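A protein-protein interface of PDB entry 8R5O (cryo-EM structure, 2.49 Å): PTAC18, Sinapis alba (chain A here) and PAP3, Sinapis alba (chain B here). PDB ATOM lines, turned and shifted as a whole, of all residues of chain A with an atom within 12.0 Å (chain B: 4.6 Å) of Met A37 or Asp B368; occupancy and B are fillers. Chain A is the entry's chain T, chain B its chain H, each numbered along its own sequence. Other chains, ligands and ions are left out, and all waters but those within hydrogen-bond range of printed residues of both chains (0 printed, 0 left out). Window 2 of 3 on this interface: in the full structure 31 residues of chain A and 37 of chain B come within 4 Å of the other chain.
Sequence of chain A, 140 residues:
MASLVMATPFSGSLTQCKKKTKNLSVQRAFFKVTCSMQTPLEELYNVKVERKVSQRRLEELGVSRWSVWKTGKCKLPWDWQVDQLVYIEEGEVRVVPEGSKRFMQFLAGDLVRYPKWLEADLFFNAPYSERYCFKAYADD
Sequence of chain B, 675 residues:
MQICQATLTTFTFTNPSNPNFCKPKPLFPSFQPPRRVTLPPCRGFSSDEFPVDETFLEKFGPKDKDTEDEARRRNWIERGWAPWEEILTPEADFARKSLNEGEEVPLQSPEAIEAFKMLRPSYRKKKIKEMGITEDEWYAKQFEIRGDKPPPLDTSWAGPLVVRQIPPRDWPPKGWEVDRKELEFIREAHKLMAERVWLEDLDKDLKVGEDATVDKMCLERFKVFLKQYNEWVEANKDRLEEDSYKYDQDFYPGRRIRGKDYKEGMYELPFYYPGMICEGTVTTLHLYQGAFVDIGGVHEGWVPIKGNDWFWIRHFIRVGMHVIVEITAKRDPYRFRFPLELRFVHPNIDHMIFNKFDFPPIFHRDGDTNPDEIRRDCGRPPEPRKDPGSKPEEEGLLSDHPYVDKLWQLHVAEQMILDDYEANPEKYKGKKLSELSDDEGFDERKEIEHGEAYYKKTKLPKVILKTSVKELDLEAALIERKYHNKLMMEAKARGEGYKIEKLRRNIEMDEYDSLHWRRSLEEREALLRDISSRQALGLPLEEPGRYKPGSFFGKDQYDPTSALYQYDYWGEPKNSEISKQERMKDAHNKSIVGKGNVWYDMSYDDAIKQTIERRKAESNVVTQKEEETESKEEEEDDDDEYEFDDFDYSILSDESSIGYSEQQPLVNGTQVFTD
The side-chain hydroxyl (OH) of Tyr A45 is in hydrogen-bond range of the side-chain amide nitrogen (ND2) of Asn B370 (3.3 Å).
The side-chain carboxylate (OE1) of Glu B373 is in salt-bridge range of the guanidinium group (NH1) of Arg A102 (3.3 Å).
NH2 of Arg B335 lies close to SD of Met A37, 3.7 Å away.
The side-chain sulfur (SD) of Met A37 lies close to the side-chain carboxylate (OD2) of Asp B377, 3.4 Å away.
The side-chain carboxylate of Asp B377 is in hydrogen-bond range of the side-chain hydroxyl of Thr A39, at 3.2 Å.
OE2 of Glu B373 lies within hydrogen-bond range of OG of Ser A100 (2.9 Å).
O of Gly A99 lies close to OD1 of Asn B370, at 3.5 Å.
ND2 of Asn B370 lies within hydrogen-bond range of O of Glu A98 (3.3 Å).
OG of Ser A100 lies within hydrogen-bond range of N of Arg A102 (3.0 Å).
The guanidinium group of Arg B335 lies within salt-bridge range of the side-chain carboxylate of Asp B368.
O of Thr A39 is in hydrogen-bond range of NH2 of Arg A102 (2.7 Å).
The side-chain amide nitrogen of Asn B370 sits close to the side-chain carboxylate of Glu B373 (3.3 Å).
OD2 of Asp B368 is in hydrogen-bond range of N of Arg B365 (2.7 Å).
The backbone carbonyl oxygen of Arg B335 lies within hydrogen-bond range of the backbone NH of Phe B363, at 2.8 Å.
Among the printed residues, pairs that only touch across the chains: Met A37 with Gly B367 (3.6 Å), Met A37 with Asp B368 (3.7 Å), Met A37 with Glu B373 (3.7 Å), Met A37 with Ile B374 (3.9 Å), Leu A41 with Glu B373 (3.8 Å), Leu A44 with Asp B377 (3.8 Å), Tyr A45 with Glu B373 (3.3 Å) and Ser A100 with Asn B370 (3.6 Å).
Met A37 touches just these residues of chain B: Arg B335, Gly B367, Asp B368, Glu B373, Ile B374 and Asp B377.
Of the printed residues of chain B, Thr A39 touches Asp B377.
Of the printed residues of chain B, Leu A41 touches Glu B373.
Glu A43 touches none of the printed residues of chain B.
Printed residues of chain B within 4 Å of Leu A44: Asp B377.
Of the printed residues of chain B, Ser A100 touches Asn B370 and Glu B373.
Lys A101 touches none of the printed residues of chain B.
Printed residues of chain B within 4 Å of Arg A102: Glu B373 (3.3 Å).
No residue of chain A comes within 4 Å of Thr B369.
Of chain A, only Tyr A45, Glu A98, Gly A99 and Ser A100 come within 4 Å of Asn B370.
The nearest printed residue of chain B that does not touch Met A37 is Asn B370 (5.3 Å).
The nearest residue of chain A that does not touch Asp B368 is Gln A38 (6.1 Å).
Hydrophobic or aromatic side chains of chain A within 4 Å of the printed part of chain B: Met A37, Leu A41, Leu A44 and Tyr A45.
Of the 12 printed residues of chain B, 7 touch a printed residue of chain A.
Along chain B the printed residues that touch a printed residue of chain A span positions 335 to 377.
Among the printed residues, 16 pairs touch across the chains.
Among the printed residues, Asp or Glu carboxylates within 4 Å of a Lys or Arg side-chain nitrogen of the other chain: Arg A102 with Glu B373 (3.3 Å).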
ATOM      1  N   MET A  37      -5.848  -2.842  18.503  1.00  0.00           N
ATOM      2  CA  MET A  37      -7.278  -2.798  18.787  1.00  0.00           C
ATOM      3  C   MET A  37      -7.547  -2.066  20.098  1.00  0.00           C
ATOM      4  O   MET A  37      -6.633  -1.510  20.706  1.00  0.00           O
ATOM      5  CB  MET A  37      -7.856  -4.212  18.842  1.00  0.00           C
ATOM      6  CG  MET A  37      -7.282  -5.079  19.950  1.00  0.00           C
ATOM      7  SD  MET A  37      -7.844  -6.786  19.845  1.00  0.00           S
ATOM      8  CE  MET A  37      -7.179  -7.258  18.252  1.00  0.00           C
ATOM      9  N   GLN A  38      -8.809  -2.069  20.528  1.00  0.00           N
ATOM     10  CA  GLN A  38      -9.178  -1.381  21.759  1.00  0.00           C
ATOM     11  C   GLN A  38      -8.764  -2.154  23.006  1.00  0.00           C
ATOM     12  O   GLN A  38      -8.418  -1.540  24.020  1.00  0.00           O
ATOM     13  CB  GLN A  38     -10.686  -1.123  21.789  1.00  0.00           C
ATOM     14  CG  GLN A  38     -11.172  -0.134  20.745  1.00  0.00           C
ATOM     15  CD  GLN A  38     -12.635   0.220  20.920  1.00  0.00           C
ATOM     16  OE1 GLN A  38     -13.345  -0.405  21.706  1.00  0.00           O
ATOM     17  NE2 GLN A  38     -13.090   1.231  20.191  1.00  0.00           N
ATOM     18  N   THR A  39      -8.798  -3.481  22.957  1.00  0.00           N
ATOM     19  CA  THR A  39      -8.512  -4.278  24.144  1.00  0.00           C
ATOM     20  C   THR A  39      -7.024  -4.219  24.473  1.00  0.00           C
ATOM     21  O   THR A  39      -6.189  -4.395  23.578  1.00  0.00           O
ATOM     22  CB  THR A  39      -8.949  -5.727  23.935  1.00  0.00           C
ATOM     23  OG1 THR A  39     -10.314  -5.759  23.503  1.00  0.00           O
ATOM     24  CG2 THR A  39      -8.826  -6.512  25.231  1.00  0.00           C
ATOM     25  N   PRO A  40      -6.654  -3.969  25.727  1.00  0.00           N
ATOM     26  CA  PRO A  40      -5.233  -3.945  26.091  1.00  0.00           C
ATOM     27  C   PRO A  40      -4.595  -5.319  25.965  1.00  0.00           C
ATOM     28  O   PRO A  40      -5.256  -6.357  26.039  1.00  0.00           O
ATOM     29  CB  PRO A  40      -5.245  -3.472  27.549  1.00  0.00           C
ATOM     30  CG  PRO A  40      -6.571  -2.808  27.730  1.00  0.00           C
ATOM     31  CD  PRO A  40      -7.516  -3.554  26.844  1.00  0.00           C
ATOM     32  N   LEU A  41      -3.273  -5.307  25.770  1.00  0.00           N
ATOM     33  CA  LEU A  41      -2.536  -6.555  25.597  1.00  0.00           C
ATOM     34  C   LEU A  41      -2.606  -7.428  26.844  1.00  0.00           C
ATOM     35  O   LEU A  41      -2.669  -8.658  26.743  1.00  0.00           O
ATOM     36  CB  LEU A  41      -1.081  -6.262  25.233  1.00  0.00           C
ATOM     37  CG  LEU A  41      -0.779  -5.753  23.824  1.00  0.00           C
ATOM     38  CD1 LEU A  41       0.718  -5.567  23.649  1.00  0.00           C
ATOM     39  CD2 LEU A  41      -1.327  -6.708  22.779  1.00  0.00           C
ATOM     40  N   GLU A  42      -2.584  -6.813  28.031  1.00  0.00           N
ATOM     41  CA  GLU A  42      -2.666  -7.587  29.265  1.00  0.00           C
ATOM     42  C   GLU A  42      -3.973  -8.364  29.345  1.00  0.00           C
ATOM     43  O   GLU A  42      -3.994  -9.515  29.792  1.00  0.00           O
ATOM     44  CB  GLU A  42      -2.520  -6.671  30.480  1.00  0.00           C
ATOM     45  CG  GLU A  42      -1.089  -6.318  30.842  1.00  0.00           C
ATOM     46  CD  GLU A  42      -0.726  -4.896  30.473  1.00  0.00           C
ATOM     47  OE1 GLU A  42      -1.060  -4.466  29.351  1.00  0.00           O
ATOM     48  OE2 GLU A  42      -0.113  -4.202  31.314  1.00  0.00           O
ATOM     49  N   GLU A  43      -5.077  -7.743  28.926  1.00  0.00           N
ATOM     50  CA  GLU A  43      -6.357  -8.442  28.916  1.00  0.00           C
ATOM     51  C   GLU A  43      -6.370  -9.557  27.878  1.00  0.00           C
ATOM     52  O   GLU A  43      -6.845 -10.664  28.155  1.00  0.00           O
ATOM     53  CB  GLU A  43      -7.490  -7.449  28.653  1.00  0.00           C
ATOM     54  CG  GLU A  43      -8.860  -7.934  29.094  1.00  0.00           C
ATOM     55  CD  GLU A  43      -9.124  -7.665  30.563  1.00  0.00           C
ATOM     56  OE1 GLU A  43      -8.696  -6.603  31.060  1.00  0.00           O
ATOM     57  OE2 GLU A  43      -9.757  -8.516  31.221  1.00  0.00           O
ATOM     58  N   LEU A  44      -5.853  -9.283  26.677  1.00  0.00           N
ATOM     59  CA  LEU A  44      -5.882 -10.273  25.606  1.00  0.00           C
ATOM     60  C   LEU A  44      -5.037 -11.496  25.944  1.00  0.00           C
ATOM     61  O   LEU A  44      -5.461 -12.634  25.715  1.00  0.00           O
ATOM     62  CB  LEU A  44      -5.397  -9.648  24.299  1.00  0.00           C
ATOM     63  CG  LEU A  44      -6.314  -8.647  23.602  1.00  0.00           C
ATOM     64  CD1 LEU A  44      -5.594  -7.996  22.434  1.00  0.00           C
ATOM     65  CD2 LEU A  44      -7.582  -9.336  23.132  1.00  0.00           C
ATOM     66  N   TYR A  45      -3.841 -11.285  26.487  1.00  0.00           N
ATOM     67  CA  TYR A  45      -2.885 -12.360  26.701  1.00  0.00           C
ATOM     68  C   TYR A  45      -2.911 -12.923  28.115  1.00  0.00           C
ATOM     69  O   TYR A  45      -2.093 -13.791  28.430  1.00  0.00           O
ATOM     70  CB  TYR A  45      -1.474 -11.881  26.353  1.00  0.00           C
ATOM     71  CG  TYR A  45      -1.243 -11.761  24.868  1.00  0.00           C
ATOM     72  CD1 TYR A  45      -0.751 -12.830  24.135  1.00  0.00           C
ATOM     73  CD2 TYR A  45      -1.535 -10.583  24.191  1.00  0.00           C
ATOM     74  CE1 TYR A  45      -0.546 -12.730  22.776  1.00  0.00           C
ATOM     75  CE2 TYR A  45      -1.334 -10.475  22.831  1.00  0.00           C
ATOM     76  CZ  TYR A  45      -0.840 -11.551  22.129  1.00  0.00           C
ATOM     77  OH  TYR A  45      -0.635 -11.450  20.772  1.00  0.00           O
ATOM     78  N   ASN A  46      -3.828 -12.456  28.965  1.00  0.00           N
ATOM     79  CA  ASN A  46      -3.989 -12.975  30.323  1.00  0.00           C
ATOM     80  C   ASN A  46      -2.691 -12.843  31.122  1.00  0.00           C
ATOM     81  O   ASN A  46      -2.212 -13.790  31.748  1.00  0.00           O
ATOM     82  CB  ASN A  46      -4.480 -14.425  30.300  1.00  0.00           C
ATOM     83  CG  ASN A  46      -4.889 -14.929  31.669  1.00  0.00           C
ATOM     84  OD1 ASN A  46      -5.401 -14.175  32.497  1.00  0.00           O
ATOM     85  ND2 ASN A  46      -4.653 -16.212  31.920  1.00  0.00           N
ATOM     86  N   PRO A  97       4.417  -9.316  22.427  1.00  0.00           N
ATOM     87  CA  PRO A  97       3.976 -10.655  22.026  1.00  0.00           C
ATOM     88  C   PRO A  97       4.273 -10.915  20.557  1.00  0.00           C
ATOM     89  O   PRO A  97       4.429  -9.995  19.753  1.00  0.00           O
ATOM     90  CB  PRO A  97       2.468 -10.632  22.298  1.00  0.00           C
ATOM     91  CG  PRO A  97       2.288  -9.559  23.318  1.00  0.00           C
ATOM     92  CD  PRO A  97       3.315  -8.520  22.992  1.00  0.00           C
ATOM     93  N   GLU A  98       4.373 -12.199  20.220  1.00  0.00           N
ATOM     94  CA  GLU A  98       4.757 -12.606  18.875  1.00  0.00           C
ATOM     95  C   GLU A  98       3.797 -12.029  17.841  1.00  0.00           C
ATOM     96  O   GLU A  98       2.585 -12.249  17.915  1.00  0.00           O
ATOM     97  CB  GLU A  98       4.787 -14.131  18.788  1.00  0.00           C
ATOM     98  CG  GLU A  98       5.844 -14.688  17.850  1.00  0.00           C
ATOM     99  CD  GLU A  98       5.483 -14.526  16.390  1.00  0.00           C
ATOM    100  OE1 GLU A  98       4.277 -14.429  16.077  1.00  0.00           O
ATOM    101  OE2 GLU A  98       6.407 -14.500  15.551  1.00  0.00           O
ATOM    102  N   GLY A  99       4.346 -11.291  16.878  1.00  0.00           N
ATOM    103  CA  GLY A  99       3.563 -10.677  15.828  1.00  0.00           C
ATOM    104  C   GLY A  99       2.900  -9.367  16.192  1.00  0.00           C
ATOM    105  O   GLY A  99       2.143  -8.830  15.373  1.00  0.00           O
ATOM    106  N   SER A 100       3.157  -8.830  17.380  1.00  0.00           N
ATOM    107  CA  SER A 100       2.471  -7.638  17.854  1.00  0.00           C
ATOM    108  C   SER A 100       3.230  -6.370  17.481  1.00  0.00           C
ATOM    109  O   SER A 100       4.453  -6.373  17.329  1.00  0.00           O
ATOM    110  CB  SER A 100       2.286  -7.695  19.371  1.00  0.00           C
ATOM    111  OG  SER A 100       1.626  -6.537  19.846  1.00  0.00           O
ATOM    112  N   LYS A 101       2.479  -5.280  17.332  1.00  0.00           N
ATOM    113  CA  LYS A 101       3.044  -3.950  17.157  1.00  0.00           C
ATOM    114  C   LYS A 101       2.995  -3.117  18.430  1.00  0.00           C
ATOM    115  O   LYS A 101       3.589  -2.036  18.467  1.00  0.00           O
ATOM    116  CB  LYS A 101       2.313  -3.198  16.036  1.00  0.00           C
ATOM    117  CG  LYS A 101       3.015  -3.239  14.688  1.00  0.00           C
ATOM    118  CD  LYS A 101       3.092  -4.651  14.135  1.00  0.00           C
ATOM    119  CE  LYS A 101       3.759  -4.669  12.770  1.00  0.00           C
ATOM    120  NZ  LYS A 101       3.835  -6.041  12.198  1.00  0.00           N
ATOM    121  N   ARG A 102       2.306  -3.589  19.460  1.00  0.00           N
ATOM    122  CA  ARG A 102       2.214  -2.918  20.747  1.00  0.00           C
ATOM    123  C   ARG A 102       3.065  -3.660  21.769  1.00  0.00           C
ATOM    124  O   ARG A 102       3.556  -4.764  21.520  1.00  0.00           O
ATOM    125  CB  ARG A 102       0.757  -2.839  21.212  1.00  0.00           C
ATOM    126  CG  ARG A 102      -0.202  -2.342  20.148  1.00  0.00           C
ATOM    127  CD  ARG A 102      -1.532  -3.071  20.222  1.00  0.00           C
ATOM    128  NE  ARG A 102      -2.274  -2.742  21.431  1.00  0.00           N
ATOM    129  CZ  ARG A 102      -3.379  -3.361  21.822  1.00  0.00           C
ATOM    130  NH1 ARG A 102      -3.888  -4.367  21.131  1.00  0.00           N
ATOM    131  NH2 ARG A 102      -3.988  -2.961  22.933  1.00  0.00           N
ATOM    132  N   PHE A 103       3.236  -3.044  22.935  1.00  0.00           N
ATOM    133  CA  PHE A 103       4.044  -3.639  23.986  1.00  0.00           C
ATOM    134  C   PHE A 103       3.364  -3.458  25.336  1.00  0.00           C
ATOM    135  O   PHE A 103       2.549  -2.556  25.533  1.00  0.00           O
ATOM    136  CB  PHE A 103       5.462  -3.044  24.019  1.00  0.00           C
ATOM    137  CG  PHE A 103       5.501  -1.561  24.276  1.00  0.00           C
ATOM    138  CD1 PHE A 103       5.567  -1.068  25.568  1.00  0.00           C
ATOM    139  CD2 PHE A 103       5.489  -0.662  23.222  1.00  0.00           C
ATOM    140  CE1 PHE A 103       5.608   0.292  25.805  1.00  0.00           C
ATOM    141  CE2 PHE A 103       5.533   0.698  23.454  1.00  0.00           C
ATOM    142  CZ  PHE A 103       5.592   1.176  24.747  1.00  0.00           C
ATOM    143  N   MET A 104       3.713  -4.346  26.261  1.00  0.00           N
ATOM    144  CA  MET A 104       3.336  -4.231  27.662  1.00  0.00           C
ATOM    145  C   MET A 104       4.552  -3.775  28.454  1.00  0.00           C
ATOM    146  O   MET A 104       5.640  -4.338  28.304  1.00  0.00           O
ATOM    147  CB  MET A 104       2.826  -5.567  28.207  1.00  0.00           C
ATOM    148  CG  MET A 104       1.504  -6.019  27.627  1.00  0.00           C
ATOM    149  SD  MET A 104       1.064  -7.695  28.123  1.00  0.00           S
ATOM    150  CE  MET A 104       2.268  -8.648  27.207  1.00  0.00           C
ATOM    151  N   ARG B 335     -16.232  -5.477  17.960  1.00  0.00           N
ATOM    152  CA  ARG B 335     -15.612  -6.667  17.392  1.00  0.00           C
ATOM    153  C   ARG B 335     -16.602  -7.531  16.622  1.00  0.00           C
ATOM    154  O   ARG B 335     -16.275  -8.021  15.537  1.00  0.00           O
ATOM    155  CB  ARG B 335     -14.950  -7.493  18.498  1.00  0.00           C
ATOM    156  CG  ARG B 335     -14.317  -8.793  18.023  1.00  0.00           C
ATOM    157  CD  ARG B 335     -13.274  -8.542  16.946  1.00  0.00           C
ATOM    158  NE  ARG B 335     -12.197  -7.685  17.422  1.00  0.00           N
ATOM    159  CZ  ARG B 335     -11.299  -7.104  16.638  1.00  0.00           C
ATOM    160  NH1 ARG B 335     -11.325  -7.258  15.325  1.00  0.00           N
ATOM    161  NH2 ARG B 335     -10.357  -6.343  17.185  1.00  0.00           N
ATOM    162  N   PHE B 363     -15.720  -8.218  12.797  1.00  0.00           N
ATOM    163  CA  PHE B 363     -15.092  -7.218  11.944  1.00  0.00           C
ATOM    164  C   PHE B 363     -13.583  -7.412  11.934  1.00  0.00           C
ATOM    165  O   PHE B 363     -12.983  -7.762  12.953  1.00  0.00           O
ATOM    166  CB  PHE B 363     -15.406  -5.800  12.427  1.00  0.00           C
ATOM    167  CG  PHE B 363     -16.826  -5.374  12.214  1.00  0.00           C
ATOM    168  CD1 PHE B 363     -17.249  -4.916  10.979  1.00  0.00           C
ATOM    169  CD2 PHE B 363     -17.733  -5.398  13.260  1.00  0.00           C
ATOM    170  CE1 PHE B 363     -18.551  -4.512  10.784  1.00  0.00           C
ATOM    171  CE2 PHE B 363     -19.036  -4.994  13.070  1.00  0.00           C
ATOM    172  CZ  PHE B 363     -19.446  -4.551  11.830  1.00  0.00           C
ATOM    173  N   HIS B 364     -12.972  -7.176  10.778  1.00  0.00           N
ATOM    174  CA  HIS B 364     -11.523  -7.053  10.656  1.00  0.00           C
ATOM    175  C   HIS B 364     -11.225  -5.584  10.385  1.00  0.00           C
ATOM    176  O   HIS B 364     -11.413  -5.105   9.261  1.00  0.00           O
ATOM    177  CB  HIS B 364     -10.983  -7.953   9.548  1.00  0.00           C
ATOM    178  CG  HIS B 364     -11.225  -9.412   9.788  1.00  0.00           C
ATOM    179  ND1 HIS B 364     -10.231 -10.274  10.193  1.00  0.00           N
ATOM    180  CD2 HIS B 364     -12.351 -10.157   9.685  1.00  0.00           C
ATOM    181  CE1 HIS B 364     -10.731 -11.489  10.326  1.00  0.00           C
ATOM    182  NE2 HIS B 364     -12.016 -11.444  10.023  1.00  0.00           N
ATOM    183  N   ARG B 365     -10.765  -4.871  11.409  1.00  0.00           N
ATOM    184  CA  ARG B 365     -10.710  -3.419  11.380  1.00  0.00           C
ATOM    185  C   ARG B 365      -9.284  -2.927  11.142  1.00  0.00           C
ATOM    186  O   ARG B 365      -8.347  -3.707  10.951  1.00  0.00           O
ATOM    187  CB  ARG B 365     -11.286  -2.846  12.676  1.00  0.00           C
ATOM    188  CG  ARG B 365     -12.585  -3.506  13.109  1.00  0.00           C
ATOM    189  CD  ARG B 365     -13.326  -2.667  14.129  1.00  0.00           C
ATOM    190  NE  ARG B 365     -14.063  -1.578  13.502  1.00  0.00           N
ATOM    191  CZ  ARG B 365     -15.384  -1.521  13.412  1.00  0.00           C
ATOM    192  NH1 ARG B 365     -16.154  -2.457  13.936  1.00  0.00           N
ATOM    193  NH2 ARG B 365     -15.946  -0.492  12.785  1.00  0.00           N
ATOM    194  N   ASP B 366      -9.126  -1.600  11.160  1.00  0.00           N
ATOM    195  CA  ASP B 366      -7.856  -0.983  10.783  1.00  0.00           C
ATOM    196  C   ASP B 366      -6.737  -1.355  11.747  1.00  0.00           C
ATOM    197  O   ASP B 366      -5.607  -1.620  11.322  1.00  0.00           O
ATOM    198  CB  ASP B 366      -8.016   0.534  10.708  1.00  0.00           C
ATOM    199  CG  ASP B 366      -8.995   0.966   9.634  1.00  0.00           C
ATOM    200  OD1 ASP B 366      -9.100   0.263   8.608  1.00  0.00           O
ATOM    201  OD2 ASP B 366      -9.661   2.007   9.817  1.00  0.00           O
ATOM    202  N   GLY B 367      -7.024  -1.380  13.042  1.00  0.00           N
ATOM    203  CA  GLY B 367      -6.007  -1.660  14.032  1.00  0.00           C
ATOM    204  C   GLY B 367      -5.696  -3.124  14.239  1.00  0.00           C
ATOM    205  O   GLY B 367      -4.871  -3.453  15.098  1.00  0.00           O
ATOM    206  N   ASP B 368      -6.323  -4.015  13.477  1.00  0.00           N
ATOM    207  CA  ASP B 368      -6.148  -5.458  13.629  1.00  0.00           C
ATOM    208  C   ASP B 368      -5.046  -5.906  12.673  1.00  0.00           C
ATOM    209  O   ASP B 368      -5.306  -6.303  11.538  1.00  0.00           O
ATOM    210  CB  ASP B 368      -7.457  -6.191  13.361  1.00  0.00           C
ATOM    211  CG  ASP B 368      -8.609  -5.644  14.177  1.00  0.00           C
ATOM    212  OD1 ASP B 368      -8.359  -5.105  15.276  1.00  0.00           O
ATOM    213  OD2 ASP B 368      -9.766  -5.752  13.720  1.00  0.00           O
ATOM    214  N   THR B 369      -3.801  -5.841  13.143  1.00  0.00           N
ATOM    215  CA  THR B 369      -2.661  -6.265  12.342  1.00  0.00           C
ATOM    216  C   THR B 369      -2.098  -7.616  12.761  1.00  0.00           C
ATOM    217  O   THR B 369      -1.464  -8.284  11.937  1.00  0.00           O
ATOM    218  CB  THR B 369      -1.542  -5.218  12.408  1.00  0.00           C
ATOM    219  OG1 THR B 369      -1.070  -5.103  13.755  1.00  0.00           O
ATOM    220  CG2 THR B 369      -2.053  -3.864  11.939  1.00  0.00           C
ATOM    221  N   ASN B 370      -2.314  -8.035  14.007  1.00  0.00           N
ATOM    222  CA  ASN B 370      -1.785  -9.301  14.487  1.00  0.00           C
ATOM    223  C   ASN B 370      -2.898 -10.337  14.506  1.00  0.00           C
ATOM    224  O   ASN B 370      -3.865 -10.177  15.266  1.00  0.00           O
ATOM    225  CB  ASN B 370      -1.181  -9.139  15.881  1.00  0.00           C
ATOM    226  CG  ASN B 370      -0.483 -10.395  16.368  1.00  0.00           C
ATOM    227  OD1 ASN B 370      -0.280 -11.343  15.610  1.00  0.00           O
ATOM    228  ND2 ASN B 370      -0.102 -10.403  17.638  1.00  0.00           N
ATOM    229  N   GLU B 373      -3.742 -11.699  18.001  1.00  0.00           N
ATOM    230  CA  GLU B 373      -4.531 -10.820  18.859  1.00  0.00           C
ATOM    231  C   GLU B 373      -6.006 -10.862  18.483  1.00  0.00           C
ATOM    232  O   GLU B 373      -6.876 -10.811  19.361  1.00  0.00           O
ATOM    233  CB  GLU B 373      -4.011  -9.389  18.777  1.00  0.00           C
ATOM    234  CG  GLU B 373      -2.618  -9.189  19.328  1.00  0.00           C
ATOM    235  CD  GLU B 373      -2.148  -7.756  19.189  1.00  0.00           C
ATOM    236  OE1 GLU B 373      -3.003  -6.846  19.217  1.00  0.00           O
ATOM    237  OE2 GLU B 373      -0.930  -7.540  19.042  1.00  0.00           O
ATOM    238  N   ILE B 374      -6.305 -10.940  17.185  1.00  0.00           N
ATOM    239  CA  ILE B 374      -7.694 -10.944  16.736  1.00  0.00           C
ATOM    240  C   ILE B 374      -8.429 -12.155  17.293  1.00  0.00           C
ATOM    241  O   ILE B 374      -9.536 -12.037  17.830  1.00  0.00           O
ATOM    242  CB  ILE B 374      -7.763 -10.909  15.199  1.00  0.00           C
ATOM    243  CG1 ILE B 374      -7.035  -9.679  14.657  1.00  0.00           C
ATOM    244  CG2 ILE B 374      -9.210 -10.925  14.731  1.00  0.00           C
ATOM    245  CD1 ILE B 374      -6.818  -9.720  13.163  1.00  0.00           C
ATOM    246  N   ASP B 377      -9.405 -11.809  20.861  1.00  0.00           N
ATOM    247  CA  ASP B 377     -10.510 -10.894  21.120  1.00  0.00           C
ATOM    248  C   ASP B 377     -11.853 -11.602  20.993  1.00  0.00           C
ATOM    249  O   ASP B 377     -12.795 -11.282  21.726  1.00  0.00           O
ATOM    250  CB  ASP B 377     -10.437  -9.699  20.171  1.00  0.00           C
ATOM    251  CG  ASP B 377     -10.978  -8.428  20.792  1.00  0.00           C
ATOM    252  OD1 ASP B 377     -11.243  -8.423  22.011  1.00  0.00           O
ATOM    253  OD2 ASP B 377     -11.138  -7.429  20.060  1.00  0.00           O
